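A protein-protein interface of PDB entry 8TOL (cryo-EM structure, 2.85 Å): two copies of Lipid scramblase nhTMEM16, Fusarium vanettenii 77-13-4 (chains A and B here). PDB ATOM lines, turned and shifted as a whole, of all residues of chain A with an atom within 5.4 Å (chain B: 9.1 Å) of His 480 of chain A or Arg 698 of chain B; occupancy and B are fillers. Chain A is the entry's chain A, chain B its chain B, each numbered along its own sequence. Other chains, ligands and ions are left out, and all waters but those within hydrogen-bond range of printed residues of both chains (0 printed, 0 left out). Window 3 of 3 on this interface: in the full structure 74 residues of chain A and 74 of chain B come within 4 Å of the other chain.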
ATOM      1  N   GLU A  56     -24.509  10.174 -12.666  1.00  0.00           N
ATOM      2  CA  GLU A  56     -23.697   8.981 -12.493  1.00  0.00           C
ATOM      3  C   GLU A  56     -23.461   8.349 -13.857  1.00  0.00           C
ATOM      4  O   GLU A  56     -24.297   8.460 -14.756  1.00  0.00           O
ATOM      5  CB  GLU A  56     -24.364   7.972 -11.553  1.00  0.00           C
ATOM      6  CG  GLU A  56     -24.476   8.445 -10.116  1.00  0.00           C
ATOM      7  CD  GLU A  56     -23.199   8.228  -9.330  1.00  0.00           C
ATOM      8  OE1 GLU A  56     -22.421   7.324  -9.700  1.00  0.00           O
ATOM      9  OE2 GLU A  56     -22.972   8.959  -8.343  1.00  0.00           O
ATOM     10  N   ARG A  58     -22.022   4.760 -15.984  1.00  0.00           N
ATOM     11  CA  ARG A  58     -21.873   3.314 -15.858  1.00  0.00           C
ATOM     12  C   ARG A  58     -21.522   2.732 -17.222  1.00  0.00           C
ATOM     13  O   ARG A  58     -21.142   3.449 -18.153  1.00  0.00           O
ATOM     14  CB  ARG A  58     -23.145   2.675 -15.285  1.00  0.00           C
ATOM     15  CG  ARG A  58     -23.478   3.082 -13.864  1.00  0.00           C
ATOM     16  CD  ARG A  58     -22.471   2.521 -12.879  1.00  0.00           C
ATOM     17  NE  ARG A  58     -22.856   2.801 -11.501  1.00  0.00           N
ATOM     18  CZ  ARG A  58     -22.655   3.961 -10.892  1.00  0.00           C
ATOM     19  NH1 ARG A  58     -22.067   4.973 -11.508  1.00  0.00           N
ATOM     20  NH2 ARG A  58     -23.054   4.109  -9.631  1.00  0.00           N
ATOM     21  N   GLU A 478     -16.567  -5.002 -16.807  1.00  0.00           N
ATOM     22  CA  GLU A 478     -16.809  -5.467 -15.447  1.00  0.00           C
ATOM     23  C   GLU A 478     -17.902  -4.644 -14.773  1.00  0.00           C
ATOM     24  O   GLU A 478     -17.884  -3.415 -14.819  1.00  0.00           O
ATOM     25  CB  GLU A 478     -15.523  -5.408 -14.622  1.00  0.00           C
ATOM     26  N   ASP A 479     -18.851  -5.332 -14.145  1.00  0.00           N
ATOM     27  CA  ASP A 479     -19.963  -4.694 -13.461  1.00  0.00           C
ATOM     28  C   ASP A 479     -19.831  -4.891 -11.956  1.00  0.00           C
ATOM     29  O   ASP A 479     -19.093  -5.760 -11.483  1.00  0.00           O
ATOM     30  CB  ASP A 479     -21.308  -5.250 -13.943  1.00  0.00           C
ATOM     31  CG  ASP A 479     -22.085  -4.250 -14.774  1.00  0.00           C
ATOM     32  OD1 ASP A 479     -21.462  -3.305 -15.303  1.00  0.00           O
ATOM     33  OD2 ASP A 479     -23.317  -4.407 -14.897  1.00  0.00           O
ATOM     34  N   HIS A 480     -20.554  -4.066 -11.208  1.00  0.00           N
ATOM     35  CA  HIS A 480     -20.514  -4.096  -9.755  1.00  0.00           C
ATOM     36  C   HIS A 480     -21.722  -4.841  -9.198  1.00  0.00           C
ATOM     37  O   HIS A 480     -22.759  -4.966  -9.855  1.00  0.00           O
ATOM     38  CB  HIS A 480     -20.464  -2.679  -9.183  1.00  0.00           C
ATOM     39  CG  HIS A 480     -19.524  -2.530  -8.028  1.00  0.00           C
ATOM     40  ND1 HIS A 480     -19.566  -3.353  -6.923  1.00  0.00           N
ATOM     41  CD2 HIS A 480     -18.509  -1.660  -7.811  1.00  0.00           C
ATOM     42  CE1 HIS A 480     -18.622  -2.992  -6.072  1.00  0.00           C
ATOM     43  NE2 HIS A 480     -17.967  -1.967  -6.587  1.00  0.00           N
ATOM     44  N   GLU A 481     -21.571  -5.335  -7.973  1.00  0.00           N
ATOM     45  CA  GLU A 481     -22.632  -6.089  -7.322  1.00  0.00           C
ATOM     46  C   GLU A 481     -23.789  -5.169  -6.940  1.00  0.00           C
ATOM     47  O   GLU A 481     -23.622  -3.956  -6.785  1.00  0.00           O
ATOM     48  CB  GLU A 481     -22.085  -6.803  -6.085  1.00  0.00           C
ATOM     49  CG  GLU A 481     -23.040  -7.795  -5.436  1.00  0.00           C
ATOM     50  CD  GLU A 481     -23.340  -8.986  -6.326  1.00  0.00           C
ATOM     51  OE1 GLU A 481     -22.474  -9.352  -7.147  1.00  0.00           O
ATOM     52  OE2 GLU A 481     -24.445  -9.555  -6.203  1.00  0.00           O
ATOM     53  N   GLU A 482     -24.976  -5.763  -6.813  1.00  0.00           N
ATOM     54  CA  GLU A 482     -26.226  -5.130  -6.398  1.00  0.00           C
ATOM     55  C   GLU A 482     -26.789  -4.180  -7.446  1.00  0.00           C
ATOM     56  O   GLU A 482     -27.860  -3.603  -7.225  1.00  0.00           O
ATOM     57  CB  GLU A 482     -26.090  -4.375  -5.067  1.00  0.00           C
ATOM     58  N   GLU A 483     -26.113  -3.995  -8.578  1.00  0.00           N
ATOM     59  CA  GLU A 483     -26.640  -3.162  -9.647  1.00  0.00           C
ATOM     60  C   GLU A 483     -26.455  -3.771 -11.028  1.00  0.00           C
ATOM     61  O   GLU A 483     -26.835  -3.133 -12.015  1.00  0.00           O
ATOM     62  CB  GLU A 483     -25.990  -1.770  -9.613  1.00  0.00           C
ATOM     63  CG  GLU A 483     -24.509  -1.767  -9.951  1.00  0.00           C
ATOM     64  CD  GLU A 483     -23.877  -0.400  -9.781  1.00  0.00           C
ATOM     65  OE1 GLU A 483     -24.351   0.375  -8.924  1.00  0.00           O
ATOM     66  OE2 GLU A 483     -22.903  -0.100 -10.502  1.00  0.00           O
ATOM     67  N   ALA A 484     -25.887  -4.975 -11.133  1.00  0.00           N
ATOM     68  CA  ALA A 484     -25.663  -5.578 -12.442  1.00  0.00           C
ATOM     69  C   ALA A 484     -26.977  -5.843 -13.165  1.00  0.00           C
ATOM     70  O   ALA A 484     -27.093  -5.588 -14.369  1.00  0.00           O
ATOM     71  CB  ALA A 484     -24.863  -6.871 -12.294  1.00  0.00           C
ATOM     72  N   ALA B 675     -26.798  15.650  -1.291  1.00  0.00           N
ATOM     73  CA  ALA B 675     -26.315  14.276  -1.388  1.00  0.00           C
ATOM     74  C   ALA B 675     -25.813  13.765  -0.042  1.00  0.00           C
ATOM     75  O   ALA B 675     -26.029  12.597   0.303  1.00  0.00           O
ATOM     76  CB  ALA B 675     -25.214  14.180  -2.445  1.00  0.00           C
ATOM     77  N   THR B 690     -28.473  -0.302   1.042  1.00  0.00           N
ATOM     78  CA  THR B 690     -27.322  -0.761   0.266  1.00  0.00           C
ATOM     79  C   THR B 690     -27.464  -0.553  -1.238  1.00  0.00           C
ATOM     80  O   THR B 690     -26.516  -0.045  -1.855  1.00  0.00           O
ATOM     81  CB  THR B 690     -27.057  -2.240   0.579  1.00  0.00           C
ATOM     82  OG1 THR B 690     -26.978  -2.423   1.998  1.00  0.00           O
ATOM     83  CG2 THR B 690     -25.754  -2.696  -0.060  1.00  0.00           C
ATOM     84  N   PRO B 691     -28.576  -0.913  -1.892  1.00  0.00           N
ATOM     85  CA  PRO B 691     -28.631  -0.762  -3.349  1.00  0.00           C
ATOM     86  C   PRO B 691     -29.312   0.505  -3.846  1.00  0.00           C
ATOM     87  O   PRO B 691     -29.414   0.707  -5.058  1.00  0.00           O
ATOM     88  CB  PRO B 691     -29.396  -2.025  -3.769  1.00  0.00           C
ATOM     89  CG  PRO B 691     -30.220  -2.430  -2.484  1.00  0.00           C
ATOM     90  CD  PRO B 691     -29.892  -1.389  -1.430  1.00  0.00           C
ATOM     91  N   GLU B 692     -29.783   1.364  -2.941  1.00  0.00           N
ATOM     92  CA  GLU B 692     -30.445   2.597  -3.356  1.00  0.00           C
ATOM     93  C   GLU B 692     -29.624   3.831  -2.982  1.00  0.00           C
ATOM     94  O   GLU B 692     -29.287   4.644  -3.848  1.00  0.00           O
ATOM     95  CB  GLU B 692     -31.849   2.674  -2.744  1.00  0.00           C
ATOM     96  CG  GLU B 692     -32.505   4.051  -2.829  1.00  0.00           C
ATOM     97  CD  GLU B 692     -32.922   4.445  -4.241  1.00  0.00           C
ATOM     98  OE1 GLU B 692     -34.138   4.614  -4.473  1.00  0.00           O
ATOM     99  OE2 GLU B 692     -32.046   4.604  -5.119  1.00  0.00           O
ATOM    100  N   GLU B 693     -29.296   3.977  -1.696  1.00  0.00           N
ATOM    101  CA  GLU B 693     -28.563   5.159  -1.253  1.00  0.00           C
ATOM    102  C   GLU B 693     -27.113   5.117  -1.714  1.00  0.00           C
ATOM    103  O   GLU B 693     -26.525   6.155  -2.039  1.00  0.00           O
ATOM    104  CB  GLU B 693     -28.640   5.297   0.269  1.00  0.00           C
ATOM    105  CG  GLU B 693     -29.990   5.770   0.787  1.00  0.00           C
ATOM    106  CD  GLU B 693     -30.876   4.632   1.248  1.00  0.00           C
ATOM    107  OE1 GLU B 693     -31.404   3.902   0.385  1.00  0.00           O
ATOM    108  OE2 GLU B 693     -31.046   4.484   2.476  1.00  0.00           O
ATOM    109  N   MET B 694     -26.519   3.928  -1.758  1.00  0.00           N
ATOM    110  CA  MET B 694     -25.125   3.785  -2.152  1.00  0.00           C
ATOM    111  C   MET B 694     -24.925   3.966  -3.653  1.00  0.00           C
ATOM    112  O   MET B 694     -23.848   4.414  -4.062  1.00  0.00           O
ATOM    113  CB  MET B 694     -24.613   2.426  -1.617  1.00  0.00           C
ATOM    114  CG  MET B 694     -23.179   1.918  -1.938  1.00  0.00           C
ATOM    115  SD  MET B 694     -22.503   1.854  -3.614  1.00  0.00           S
ATOM    116  CE  MET B 694     -23.854   1.064  -4.498  1.00  0.00           C
ATOM    117  N   PHE B 695     -25.944   3.696  -4.473  1.00  0.00           N
ATOM    118  CA  PHE B 695     -25.797   3.847  -5.920  1.00  0.00           C
ATOM    119  C   PHE B 695     -25.492   5.283  -6.325  1.00  0.00           C
ATOM    120  O   PHE B 695     -24.621   5.510  -7.172  1.00  0.00           O
ATOM    121  CB  PHE B 695     -27.065   3.364  -6.626  1.00  0.00           C
ATOM    122  CG  PHE B 695     -27.085   3.643  -8.105  1.00  0.00           C
ATOM    123  CD1 PHE B 695     -26.308   2.900  -8.978  1.00  0.00           C
ATOM    124  CD2 PHE B 695     -27.891   4.644  -8.623  1.00  0.00           C
ATOM    125  CE1 PHE B 695     -26.333   3.156 -10.341  1.00  0.00           C
ATOM    126  CE2 PHE B 695     -27.923   4.906  -9.987  1.00  0.00           C
ATOM    127  CZ  PHE B 695     -27.140   4.159 -10.847  1.00  0.00           C
ATOM    128  N   TRP B 696     -26.186   6.258  -5.739  1.00  0.00           N
ATOM    129  CA  TRP B 696     -26.008   7.658  -6.109  1.00  0.00           C
ATOM    130  C   TRP B 696     -24.867   8.345  -5.376  1.00  0.00           C
ATOM    131  O   TRP B 696     -24.498   9.461  -5.759  1.00  0.00           O
ATOM    132  CB  TRP B 696     -27.301   8.448  -5.872  1.00  0.00           C
ATOM    133  CG  TRP B 696     -28.339   8.200  -6.911  1.00  0.00           C
ATOM    134  CD1 TRP B 696     -29.417   7.377  -6.812  1.00  0.00           C
ATOM    135  CD2 TRP B 696     -28.390   8.774  -8.221  1.00  0.00           C
ATOM    136  NE1 TRP B 696     -30.140   7.402  -7.976  1.00  0.00           N
ATOM    137  CE2 TRP B 696     -29.529   8.253  -8.858  1.00  0.00           C
ATOM    138  CE3 TRP B 696     -27.583   9.678  -8.914  1.00  0.00           C
ATOM    139  CZ2 TRP B 696     -29.883   8.605 -10.154  1.00  0.00           C
ATOM    140  CZ3 TRP B 696     -27.934  10.025 -10.200  1.00  0.00           C
ATOM    141  CH2 TRP B 696     -29.074   9.491 -10.806  1.00  0.00           C
ATOM    142  N   GLN B 697     -24.296   7.721  -4.349  1.00  0.00           N
ATOM    143  CA  GLN B 697     -23.201   8.313  -3.597  1.00  0.00           C
ATOM    144  C   GLN B 697     -21.832   7.844  -4.069  1.00  0.00           C
ATOM    145  O   GLN B 697     -20.820   8.222  -3.470  1.00  0.00           O
ATOM    146  CB  GLN B 697     -23.370   8.018  -2.104  1.00  0.00           C
ATOM    147  CG  GLN B 697     -22.967   6.619  -1.692  1.00  0.00           C
ATOM    148  CD  GLN B 697     -22.275   6.596  -0.349  1.00  0.00           C
ATOM    149  OE1 GLN B 697     -21.565   7.536   0.012  1.00  0.00           O
ATOM    150  NE2 GLN B 697     -22.480   5.523   0.403  1.00  0.00           N
ATOM    151  N   ARG B 698     -21.775   7.030  -5.126  1.00  0.00           N
ATOM    152  CA  ARG B 698     -20.489   6.577  -5.642  1.00  0.00           C
ATOM    153  C   ARG B 698     -19.661   7.743  -6.165  1.00  0.00           C
ATOM    154  O   ARG B 698     -18.450   7.813  -5.919  1.00  0.00           O
ATOM    155  CB  ARG B 698     -20.704   5.537  -6.739  1.00  0.00           C
ATOM    156  CG  ARG B 698     -21.277   4.225  -6.240  1.00  0.00           C
ATOM    157  CD  ARG B 698     -20.823   3.073  -7.110  1.00  0.00           C
ATOM    158  NE  ARG B 698     -21.193   1.781  -6.547  1.00  0.00           N
ATOM    159  CZ  ARG B 698     -21.049   0.624  -7.177  1.00  0.00           C
ATOM    160  NH1 ARG B 698     -20.557   0.563  -8.403  1.00  0.00           N
ATOM    161  NH2 ARG B 698     -21.407  -0.499  -6.562  1.00  0.00           N
ATOM    162  N   GLN B 699     -20.292   8.668  -6.892  1.00  0.00           N
ATOM    163  CA  GLN B 699     -19.631   9.876  -7.392  1.00  0.00           C
ATOM    164  C   GLN B 699     -20.489  11.073  -6.984  1.00  0.00           C
ATOM    165  O   GLN B 699     -21.303  11.569  -7.767  1.00  0.00           O
ATOM    166  CB  GLN B 699     -19.430   9.813  -8.906  1.00  0.00           C
ATOM    167  CG  GLN B 699     -19.138   8.426  -9.449  1.00  0.00           C
ATOM    168  CD  GLN B 699     -19.750   8.195 -10.818  1.00  0.00           C
ATOM    169  OE1 GLN B 699     -20.315   9.107 -11.419  1.00  0.00           O
ATOM    170  NE2 GLN B 699     -19.632   6.972 -11.319  1.00  0.00           N
ATOM    171  N   ARG B 700     -20.298  11.537  -5.753  1.00  0.00           N
ATOM    172  CA  ARG B 700     -21.011  12.711  -5.250  1.00  0.00           C
ATOM    173  C   ARG B 700     -20.196  13.983  -5.454  1.00  0.00           C
ATOM    174  O   ARG B 700     -19.960  14.753  -4.525  1.00  0.00           O
ATOM    175  CB  ARG B 700     -21.362  12.514  -3.780  1.00  0.00           C
ATOM    176  N   GLY B 701     -19.755  14.204  -6.684  1.00  0.00           N
ATOM    177  CA  GLY B 701     -18.956  15.373  -6.989  1.00  0.00           C
ATOM    178  C   GLY B 701     -18.667  15.438  -8.472  1.00  0.00           C
ATOM    179  O   GLY B 701     -18.698  14.428  -9.181  1.00  0.00           O
ATOM    180  N   GLU B 704     -14.807  13.987  -9.285  1.00  0.00           N
ATOM    181  CA  GLU B 704     -14.732  12.531  -9.253  1.00  0.00           C
ATOM    182  C   GLU B 704     -15.550  11.914 -10.380  1.00  0.00           C
ATOM    183  O   GLU B 704     -15.144  10.903 -10.960  1.00  0.00           O
ATOM    184  CB  GLU B 704     -15.183  12.003  -7.892  1.00  0.00           C
ATOM    185  CG  GLU B 704     -16.538  12.493  -7.424  1.00  0.00           C
ATOM    186  CD  GLU B 704     -16.716  12.330  -5.927  1.00  0.00           C
ATOM    187  OE1 GLU B 704     -15.707  12.412  -5.195  1.00  0.00           O
ATOM    188  OE2 GLU B 704     -17.859  12.103  -5.482  1.00  0.00           O
ATOM    189  N   THR B 705     -16.696  12.512 -10.709  1.00  0.00           N
ATOM    190  CA  THR B 705     -17.486  12.019 -11.833  1.00  0.00           C
ATOM    191  C   THR B 705     -16.711  12.140 -13.138  1.00  0.00           C
ATOM    192  O   THR B 705     -16.689  11.211 -13.951  1.00  0.00           O
ATOM    193  CB  THR B 705     -18.810  12.780 -11.924  1.00  0.00           C
ATOM    194  OG1 THR B 705     -19.677  12.368 -10.860  1.00  0.00           O
ATOM    195  CG2 THR B 705     -19.495  12.507 -13.254  1.00  0.00           C
ATOM    196  N   ILE B 708     -13.821   9.515 -13.112  1.00  0.00           N
ATOM    197  CA  ILE B 708     -14.295   8.153 -13.317  1.00  0.00           C
ATOM    198  C   ILE B 708     -14.818   7.979 -14.735  1.00  0.00           C
ATOM    199  O   ILE B 708     -14.667   6.907 -15.322  1.00  0.00           O
ATOM    200  CB  ILE B 708     -15.346   7.770 -12.255  1.00  0.00           C
ATOM    201  CG1 ILE B 708     -15.501   6.251 -12.182  1.00  0.00           C
ATOM    202  CG2 ILE B 708     -16.689   8.414 -12.540  1.00  0.00           C
ATOM    203  CD1 ILE B 708     -15.688   5.726 -10.777  1.00  0.00           C
ATOM    204  N   MET B 712     -13.317   5.427 -17.322  1.00  0.00           N
ATOM    205  CA  MET B 712     -14.285   4.522 -17.919  1.00  0.00           C
ATOM    206  C   MET B 712     -14.137   4.481 -19.434  1.00  0.00           C
ATOM    207  O   MET B 712     -14.192   3.411 -20.044  1.00  0.00           O
ATOM    208  CB  MET B 712     -15.690   4.969 -17.522  1.00  0.00           C
ATOM    209  CG  MET B 712     -16.785   4.079 -18.017  1.00  0.00           C
ATOM    210  SD  MET B 712     -17.368   3.039 -16.677  1.00  0.00           S
ATOM    211  CE  MET B 712     -18.206   1.785 -17.621  1.00  0.00           C
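No position is printed for both chains.
No residue of chain B comes within 4 Å of Asp 479 of chain A.
Of chain B, only Arg 698 (3.1 Å) comes within 4 Å of His 480 of chain A.
Glu 482 of chain A touches none of the printed residues of chain B.
Printed residues of chain A within 4 Å of Trp 696 of chain B: Glu 56 (3.0 Å).
Of the printed residues of chain A, Arg 698 of chain B touches Glu 56 (3.9 Å), Arg 58 (3.5 Å), His 480 (3.1 Å) and Glu 483 (3.2 Å).
Of the printed residues of chain A, Gln 699 of chain B touches Glu 56 and Arg 58.
Of the printed residues of chain A, Met 712 of chain B touches Arg 58 (3.4 Å).
The nearest residue of chain B that does not touch His 480 of chain A is Met 694 of chain B (6.6 Å).
The nearest residue of chain A that does not touch Arg 698 of chain B is Glu 481 of chain A (4.1 Å).
The nearest printed residue of chain B that does not touch Arg 58 of chain A is Trp 696 of chain B (5.4 Å).
Among the printed residues, pairs that only touch across the chains: Glu 483 of chain A with Phe 695 of chain B, Arg 58 of chain A with Met 712 of chain B, Arg 58 of chain A with Arg 698 of chain B, Glu 56 of chain A with Phe 695 of chain B and Glu 56 of chain A with Arg 698 of chain B.
The side-chain sulfur (SD) of Met 694 of chain B sits at hydrogen-bond distance from the guanidinium group (NE) of Arg 698 of chain B (3.2 Å).
The side-chain carboxylate of Glu 483 of chain A is in salt-bridge range of the guanidinium group of Arg 58 of chain A (3.1 Å).
The side-chain hydroxyl (OG1) of Thr 705 of chain B sits close to the side-chain amide oxygen (OE1) of Gln 699 of chain B, at 3.4 Å.
The side-chain carboxylate of Glu 56 of chain A is in salt-bridge range of the guanidinium group of Arg 58 of chain A (3.0 Å).
N of Gln 699 of chain B sits at hydrogen-bond distance from OE2 of Glu 56 of chain A (3.1 Å).
OE2 of Glu 483 of chain A lies within salt-bridge range of NH1 of Arg 698 of chain B, at 3.2 Å.
O of Phe 695 of chain B sits at hydrogen-bond distance from NH2 of Arg 58 of chain A (3.2 Å).
ND1 of His 480 of chain A lies close to NH2 of Arg 698 of chain B, at 3.4 Å.
OE2 of Glu 56 of chain A lies close to O of Trp 696 of chain B, 3.0 Å away.
The guanidinium group (NH1) of Arg 58 of chain A sits close to the side-chain amide nitrogen (NE2) of Gln 699 of chain B.
Of the 17 printed residues of chain B, 5 touch a printed residue of chain A.
Printed residues of chain B that touch a printed residue of chain A: Phe 695, Trp 696, Arg 698, Gln 699 and Met 712.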
